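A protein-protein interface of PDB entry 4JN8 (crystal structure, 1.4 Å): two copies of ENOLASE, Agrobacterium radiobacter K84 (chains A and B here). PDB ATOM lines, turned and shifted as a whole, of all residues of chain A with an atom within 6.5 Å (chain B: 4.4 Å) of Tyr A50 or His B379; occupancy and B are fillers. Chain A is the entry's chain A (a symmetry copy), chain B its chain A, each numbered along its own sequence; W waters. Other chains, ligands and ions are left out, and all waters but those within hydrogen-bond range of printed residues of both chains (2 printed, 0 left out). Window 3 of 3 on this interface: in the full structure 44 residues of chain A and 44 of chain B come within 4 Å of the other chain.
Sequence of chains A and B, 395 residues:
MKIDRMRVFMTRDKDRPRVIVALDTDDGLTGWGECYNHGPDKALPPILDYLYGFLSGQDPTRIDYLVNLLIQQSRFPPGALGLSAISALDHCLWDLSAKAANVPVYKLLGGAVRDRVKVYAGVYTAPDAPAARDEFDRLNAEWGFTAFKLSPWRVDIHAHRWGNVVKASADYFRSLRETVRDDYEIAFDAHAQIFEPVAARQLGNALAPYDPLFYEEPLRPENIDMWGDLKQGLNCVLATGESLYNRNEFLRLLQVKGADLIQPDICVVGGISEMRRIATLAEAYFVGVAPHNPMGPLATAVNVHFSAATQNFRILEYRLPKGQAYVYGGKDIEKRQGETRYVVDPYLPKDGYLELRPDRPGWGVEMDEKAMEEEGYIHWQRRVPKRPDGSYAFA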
ATOM      1  N   MET A   6     -11.394 -14.024  15.937  1.00  0.00           N
ATOM      2  CA  MET A   6     -11.378 -14.143  14.494  1.00  0.00           C
ATOM      3  C   MET A   6     -11.647 -12.763  13.913  1.00  0.00           C
ATOM      4  O   MET A   6     -12.525 -12.044  14.401  1.00  0.00           O
ATOM      5  CB  MET A   6     -12.441 -15.124  14.005  1.00  0.00           C
ATOM      6  CG  MET A   6     -12.512 -15.247  12.483  1.00  0.00           C
ATOM      7  SD  MET A   6     -13.788 -16.393  11.905  1.00  0.00           S
ATOM      8  CE  MET A   6     -15.258 -15.510  12.396  1.00  0.00           C
ATOM      9  N   PRO A  45     -18.870 -14.242   5.586  1.00  0.00           N
ATOM     10  CA  PRO A  45     -18.760 -13.833   6.994  1.00  0.00           C
ATOM     11  C   PRO A  45     -19.761 -14.508   7.947  1.00  0.00           C
ATOM     12  O   PRO A  45     -19.350 -14.955   9.016  1.00  0.00           O
ATOM     13  CB  PRO A  45     -18.935 -12.311   6.928  1.00  0.00           C
ATOM     14  CG  PRO A  45     -18.387 -11.968   5.559  1.00  0.00           C
ATOM     15  CD  PRO A  45     -18.909 -13.072   4.683  1.00  0.00           C
ATOM     16  N   PRO A  46     -21.045 -14.632   7.566  1.00  0.00           N
ATOM     17  CA  PRO A  46     -21.913 -15.361   8.513  1.00  0.00           C
ATOM     18  C   PRO A  46     -21.577 -16.852   8.687  1.00  0.00           C
ATOM     19  O   PRO A  46     -21.781 -17.423   9.746  1.00  0.00           O
ATOM     20  CB  PRO A  46     -23.325 -15.175   7.942  1.00  0.00           C
ATOM     21  CG  PRO A  46     -23.155 -14.554   6.612  1.00  0.00           C
ATOM     22  CD  PRO A  46     -21.810 -13.899   6.555  1.00  0.00           C
ATOM     23  N   ILE A  47     -21.073 -17.496   7.639  1.00  0.00           N
ATOM     24  CA  ILE A  47     -20.643 -18.883   7.768  1.00  0.00           C
ATOM     25  C   ILE A  47     -19.467 -18.937   8.729  1.00  0.00           C
ATOM     26  O   ILE A  47     -19.415 -19.763   9.639  1.00  0.00           O
ATOM     27  CB  ILE A  47     -20.246 -19.476   6.406  1.00  0.00           C
ATOM     28  CG1 ILE A  47     -21.453 -19.517   5.457  1.00  0.00           C
ATOM     29  CG2 ILE A  47     -19.670 -20.857   6.591  1.00  0.00           C
ATOM     30  CD1 ILE A  47     -21.088 -19.825   4.014  1.00  0.00           C
ATOM     31  N   LEU A  48     -18.508 -18.040   8.517  1.00  0.00           N
ATOM     32  CA  LEU A  48     -17.325 -17.997   9.368  1.00  0.00           C
ATOM     33  C   LEU A  48     -17.690 -17.730  10.825  1.00  0.00           C
ATOM     34  O   LEU A  48     -17.123 -18.348  11.724  1.00  0.00           O
ATOM     35  CB  LEU A  48     -16.344 -16.946   8.836  1.00  0.00           C
ATOM     36  CG  LEU A  48     -15.656 -17.346   7.526  1.00  0.00           C
ATOM     37  CD1 LEU A  48     -15.113 -16.143   6.789  1.00  0.00           C
ATOM     38  CD2 LEU A  48     -14.532 -18.339   7.778  1.00  0.00           C
ATOM     39  N   ASP A  49     -18.634 -16.821  11.070  1.00  0.00           N
ATOM     40  CA  ASP A  49     -19.062 -16.543  12.435  1.00  0.00           C
ATOM     41  C   ASP A  49     -19.588 -17.805  13.104  1.00  0.00           C
ATOM     42  O   ASP A  49     -19.328 -18.072  14.279  1.00  0.00           O
ATOM     43  CB  ASP A  49     -20.182 -15.509  12.430  1.00  0.00           C
ATOM     44  CG  ASP A  49     -19.711 -14.106  12.098  1.00  0.00           C
ATOM     45  OD1 ASP A  49     -18.494 -13.806  12.230  1.00  0.00           O
ATOM     46  OD2 ASP A  49     -20.591 -13.294  11.729  1.00  0.00           O
ATOM     47  N   TYR A  50     -20.384 -18.563  12.366  1.00  0.00           N
ATOM     48  CA  TYR A  50     -20.966 -19.791  12.890  1.00  0.00           C
ATOM     49  C   TYR A  50     -19.870 -20.831  13.178  1.00  0.00           C
ATOM     50  O   TYR A  50     -19.851 -21.476  14.219  1.00  0.00           O
ATOM     51  CB  TYR A  50     -21.969 -20.319  11.856  1.00  0.00           C
ATOM     52  CG  TYR A  50     -22.818 -21.495  12.269  1.00  0.00           C
ATOM     53  CD1 TYR A  50     -24.025 -21.313  12.940  1.00  0.00           C
ATOM     54  CD2 TYR A  50     -22.439 -22.781  11.957  1.00  0.00           C
ATOM     55  CE1 TYR A  50     -24.823 -22.390  13.290  1.00  0.00           C
ATOM     56  CE2 TYR A  50     -23.228 -23.864  12.316  1.00  0.00           C
ATOM     57  CZ  TYR A  50     -24.427 -23.661  12.956  1.00  0.00           C
ATOM     58  OH  TYR A  50     -25.202 -24.754  13.282  1.00  0.00           O
ATOM     59  N   LEU A  51     -18.956 -21.005  12.235  1.00  0.00           N
ATOM     60  CA  LEU A  51     -17.872 -21.963  12.414  1.00  0.00           C
ATOM     61  C   LEU A  51     -16.969 -21.569  13.571  1.00  0.00           C
ATOM     62  O   LEU A  51     -16.452 -22.432  14.281  1.00  0.00           O
ATOM     63  CB  LEU A  51     -17.062 -22.080  11.120  1.00  0.00           C
ATOM     64  CG  LEU A  51     -17.809 -22.678   9.929  1.00  0.00           C
ATOM     65  CD1 LEU A  51     -16.935 -22.632   8.702  1.00  0.00           C
ATOM     66  CD2 LEU A  51     -18.276 -24.114  10.213  1.00  0.00           C
ATOM     67  N   TYR A  52     -16.764 -20.274  13.757  1.00  0.00           N
ATOM     68  CA  TYR A  52     -15.872 -19.826  14.815  1.00  0.00           C
ATOM     69  C   TYR A  52     -16.344 -20.288  16.187  1.00  0.00           C
ATOM     70  O   TYR A  52     -15.542 -20.482  17.095  1.00  0.00           O
ATOM     71  CB  TYR A  52     -15.701 -18.301  14.775  1.00  0.00           C
ATOM     72  CG  TYR A  52     -14.785 -17.822  15.875  1.00  0.00           C
ATOM     73  CD1 TYR A  52     -13.407 -18.024  15.801  1.00  0.00           C
ATOM     74  CD2 TYR A  52     -15.299 -17.220  17.014  1.00  0.00           C
ATOM     75  CE1 TYR A  52     -12.566 -17.620  16.829  1.00  0.00           C
ATOM     76  CE2 TYR A  52     -14.458 -16.814  18.044  1.00  0.00           C
ATOM     77  CZ  TYR A  52     -13.100 -17.029  17.929  1.00  0.00           C
ATOM     78  OH  TYR A  52     -12.256 -16.641  18.950  1.00  0.00           O
ATOM     79  N   GLY A  53     -17.648 -20.464  16.361  1.00  0.00           N
ATOM     80  CA  GLY A  53     -18.159 -20.972  17.628  1.00  0.00           C
ATOM     81  C   GLY A  53     -17.553 -22.306  18.042  1.00  0.00           C
ATOM     82  O   GLY A  53     -17.528 -22.645  19.217  1.00  0.00           O
ATOM     83  N   PHE A  54     -17.109 -23.095  17.071  1.00  0.00           N
ATOM     84  CA  PHE A  54     -16.484 -24.390  17.331  1.00  0.00           C
ATOM     85  C   PHE A  54     -14.969 -24.285  17.550  1.00  0.00           C
ATOM     86  O   PHE A  54     -14.324 -25.265  17.933  1.00  0.00           O
ATOM     87  CB  PHE A  54     -16.750 -25.359  16.160  1.00  0.00           C
ATOM     88  CG  PHE A  54     -18.209 -25.635  15.928  1.00  0.00           C
ATOM     89  CD1 PHE A  54     -18.830 -26.702  16.550  1.00  0.00           C
ATOM     90  CD2 PHE A  54     -18.951 -24.833  15.089  1.00  0.00           C
ATOM     91  CE1 PHE A  54     -20.173 -26.963  16.335  1.00  0.00           C
ATOM     92  CE2 PHE A  54     -20.302 -25.087  14.883  1.00  0.00           C
ATOM     93  CZ  PHE A  54     -20.898 -26.147  15.527  1.00  0.00           C
ATOM     94  N   LEU A  55     -14.397 -23.125  17.245  1.00  0.00           N
ATOM     95  CA  LEU A  55     -12.960 -22.905  17.364  1.00  0.00           C
ATOM     96  C   LEU A  55     -12.556 -22.080  18.585  1.00  0.00           C
ATOM     97  O   LEU A  55     -11.437 -22.227  19.093  1.00  0.00           O
ATOM     98  CB  LEU A  55     -12.418 -22.198  16.125  1.00  0.00           C
ATOM     99  CG  LEU A  55     -12.647 -22.914  14.801  1.00  0.00           C
ATOM    100  CD1 LEU A  55     -12.066 -22.064  13.683  1.00  0.00           C
ATOM    101  CD2 LEU A  55     -12.029 -24.306  14.838  1.00  0.00           C
ATOM    102  N   LEU A  70     -15.314 -29.005  12.252  1.00  0.00           N
ATOM    103  CA  LEU A  70     -16.061 -28.116  11.359  1.00  0.00           C
ATOM    104  C   LEU A  70     -16.815 -28.875  10.273  1.00  0.00           C
ATOM    105  O   LEU A  70     -17.945 -28.516   9.916  1.00  0.00           O
ATOM    106  CB  LEU A  70     -15.138 -27.097  10.716  1.00  0.00           C
ATOM    107  CG  LEU A  70     -14.361 -26.176  11.664  1.00  0.00           C
ATOM    108  CD1 LEU A  70     -13.642 -25.130  10.853  1.00  0.00           C
ATOM    109  CD2 LEU A  70     -15.296 -25.551  12.708  1.00  0.00           C
ATOM    110  N   GLN A  73     -19.830 -31.006  12.104  1.00  0.00           N
ATOM    111  CA  GLN A  73     -20.964 -30.306  12.696  1.00  0.00           C
ATOM    112  C   GLN A  73     -22.076 -30.021  11.698  1.00  0.00           C
ATOM    113  O   GLN A  73     -23.229 -29.859  12.090  1.00  0.00           O
ATOM    114  CB  GLN A  73     -20.548 -29.039  13.426  1.00  0.00           C
ATOM    115  CG  GLN A  73     -19.854 -28.025  12.614  1.00  0.00           C
ATOM    116  CD  GLN A  73     -20.785 -27.246  11.711  1.00  0.00           C
ATOM    117  OE1 GLN A  73     -21.962 -27.047  12.027  1.00  0.00           O
ATOM    118  NE2 GLN A  73     -20.268 -26.802  10.574  1.00  0.00           N
ATOM    119  N   GLY B  39     -27.631 -24.796   9.078  1.00  0.00           N
ATOM    120  CA  GLY B  39     -27.026 -24.337  10.312  1.00  0.00           C
ATOM    121  C   GLY B  39     -26.906 -22.833  10.333  1.00  0.00           C
ATOM    122  O   GLY B  39     -27.692 -22.148  11.006  1.00  0.00           O
ATOM    123  N   PRO B  40     -25.946 -22.298   9.572  1.00  0.00           N
ATOM    124  CA  PRO B  40     -25.692 -20.857   9.544  1.00  0.00           C
ATOM    125  C   PRO B  40     -26.686 -20.120   8.657  1.00  0.00           C
ATOM    126  O   PRO B  40     -26.321 -19.618   7.593  1.00  0.00           O
ATOM    127  CB  PRO B  40     -24.285 -20.765   8.971  1.00  0.00           C
ATOM    128  CG  PRO B  40     -24.189 -21.966   8.064  1.00  0.00           C
ATOM    129  CD  PRO B  40     -24.948 -23.052   8.790  1.00  0.00           C
ATOM    130  N   TYR B 377     -34.770 -15.045  13.914  1.00  0.00           N
ATOM    131  CA  TYR B 377     -33.698 -16.020  13.976  1.00  0.00           C
ATOM    132  C   TYR B 377     -33.464 -16.540  15.376  1.00  0.00           C
ATOM    133  O   TYR B 377     -33.605 -15.805  16.357  1.00  0.00           O
ATOM    134  CB  TYR B 377     -32.425 -15.341  13.491  1.00  0.00           C
ATOM    135  CG  TYR B 377     -31.175 -16.174  13.510  1.00  0.00           C
ATOM    136  CD1 TYR B 377     -30.893 -17.041  12.468  1.00  0.00           C
ATOM    137  CD2 TYR B 377     -30.257 -16.073  14.548  1.00  0.00           C
ATOM    138  CE1 TYR B 377     -29.745 -17.783  12.461  1.00  0.00           C
ATOM    139  CE2 TYR B 377     -29.105 -16.819  14.552  1.00  0.00           C
ATOM    140  CZ  TYR B 377     -28.846 -17.670  13.497  1.00  0.00           C
ATOM    141  OH  TYR B 377     -27.703 -18.417  13.454  1.00  0.00           O
ATOM    142  N   ILE B 378     -33.079 -17.804  15.456  1.00  0.00           N
ATOM    143  CA  ILE B 378     -32.572 -18.407  16.670  1.00  0.00           C
ATOM    144  C   ILE B 378     -31.373 -19.267  16.287  1.00  0.00           C
ATOM    145  O   ILE B 378     -31.406 -19.938  15.257  1.00  0.00           O
ATOM    146  CB  ILE B 378     -33.674 -19.236  17.378  1.00  0.00           C
ATOM    147  CG1 ILE B 378     -33.169 -19.804  18.705  1.00  0.00           C
ATOM    148  CG2 ILE B 378     -34.213 -20.354  16.474  1.00  0.00           C
ATOM    149  CD1 ILE B 378     -34.271 -20.452  19.533  1.00  0.00           C
ATOM    150  N   HIS B 379     -30.320 -19.244  17.098  1.00  0.00           N
ATOM    151  CA  HIS B 379     -29.128 -20.040  16.841  1.00  0.00           C
ATOM    152  C   HIS B 379     -29.409 -21.502  17.116  1.00  0.00           C
ATOM    153  O   HIS B 379     -29.991 -21.855  18.146  1.00  0.00           O
ATOM    154  CB  HIS B 379     -27.964 -19.578  17.716  1.00  0.00           C
ATOM    155  CG  HIS B 379     -26.731 -20.405  17.555  1.00  0.00           C
ATOM    156  ND1 HIS B 379     -25.747 -20.084  16.646  1.00  0.00           N
ATOM    157  CD2 HIS B 379     -26.337 -21.546  18.158  1.00  0.00           C
ATOM    158  CE1 HIS B 379     -24.792 -20.993  16.706  1.00  0.00           C
ATOM    159  NE2 HIS B 379     -25.121 -21.892  17.609  1.00  0.00           N
ATOM    160  N   TRP B 380     -28.973 -22.361  16.200  1.00  0.00           N
ATOM    161  CA  TRP B 380     -29.084 -23.791  16.360  1.00  0.00           C
ATOM    162  C   TRP B 380     -27.842 -24.467  15.799  1.00  0.00           C
ATOM    163  O   TRP B 380     -27.354 -24.077  14.731  1.00  0.00           O
ATOM    164  CB  TRP B 380     -30.330 -24.308  15.643  1.00  0.00           C
ATOM    165  CG  TRP B 380     -30.538 -25.790  15.715  1.00  0.00           C
ATOM    166  CD1 TRP B 380     -31.200 -26.491  16.694  1.00  0.00           C
ATOM    167  CD2 TRP B 380     -30.103 -26.762  14.759  1.00  0.00           C
ATOM    168  NE1 TRP B 380     -31.189 -27.836  16.402  1.00  0.00           N
ATOM    169  CE2 TRP B 380     -30.532 -28.029  15.214  1.00  0.00           C
ATOM    170  CE3 TRP B 380     -29.385 -26.684  13.559  1.00  0.00           C
ATOM    171  CZ2 TRP B 380     -30.272 -29.200  14.508  1.00  0.00           C
ATOM    172  CZ3 TRP B 380     -29.127 -27.850  12.864  1.00  0.00           C
ATOM    173  CH2 TRP B 380     -29.572 -29.089  13.340  1.00  0.00           C
ATOM    174  N   GLN B 381     -27.343 -25.470  16.500  1.00  0.00           N
ATOM    175  CA  GLN B 381     -26.217 -26.253  15.997  1.00  0.00           C
ATOM    176  C   GLN B 381     -26.338 -27.668  16.480  1.00  0.00           C
ATOM    177  O   GLN B 381     -27.027 -27.950  17.469  1.00  0.00           O
ATOM    178  CB  GLN B 381     -24.877 -25.642  16.416  1.00  0.00           C
ATOM    179  CG  GLN B 381     -24.606 -25.637  17.913  1.00  0.00           C
ATOM    180  CD  GLN B 381     -23.343 -24.858  18.261  1.00  0.00           C
ATOM    181  OE1 GLN B 381     -23.231 -23.675  17.967  1.00  0.00           O
ATOM    182  NE2 GLN B 381     -22.350 -25.559  18.815  1.00  0.00           N
HETATM  183  O   HOH W   1     -21.618 -21.433  16.330  1.00  0.00           O
HETATM  184  O   HOH W   2     -19.803 -24.738  19.963  1.00  0.00           O
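The backbone carbonyl oxygen (O) of Trp B380 is in hydrogen-bond range of the side-chain hydroxyl (OH) of Tyr A50, 2.7 Å away.
The side-chain amide oxygen (OE1) of Gln B381 is in hydrogen-bond range of a ring nitrogen (NE2) of His B379 (2.6 Å).
Among the printed residues, merely in contact across the chains: Tyr A50 with Gly B39, Tyr A50 with Pro B40, Tyr A50 with His B379, Tyr A50 with Gln B381 and Phe A54 with Gln B381.
Of the printed residues of chain B, Tyr A50 touches Gly B39, Pro B40, His B379, Trp B380 and Gln B381.
Tyr A52 touches none of the printed residues of chain B.
Of the printed residues of chain B, Phe A54 touches Gln B381.
Of the printed residues of chain A, Gly B39 touches Tyr A50.
Tyr B377 touches none of the printed residues of chain A.
Of chain A, only Tyr A50 comes within 4 Å of His B379.
Printed residues of chain A within 4 Å of Trp B380: Tyr A50.
The nearest printed residue of chain B that does not touch Tyr A50 is Tyr B377 (4.7 Å).
The nearest residue of chain A that does not touch His B379 is Phe A54 (6.3 Å).
Hydrophobic or aromatic side chains of chain B that line the printed part of chain A: Pro B40 and His B379.
No position is printed for both chains.
Of the 6 pairs that touch across the chains among the printed residues, none has its exchanged pair printed and touching as well.
Water W1 lies within hydrogen-bond range of O of Tyr A50 and OE1 of Gln B381.
Water W2 lies within hydrogen-bond range of NE2 of Gln B381 (2.9 Å) and O of Gly A53 (3.2 Å).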
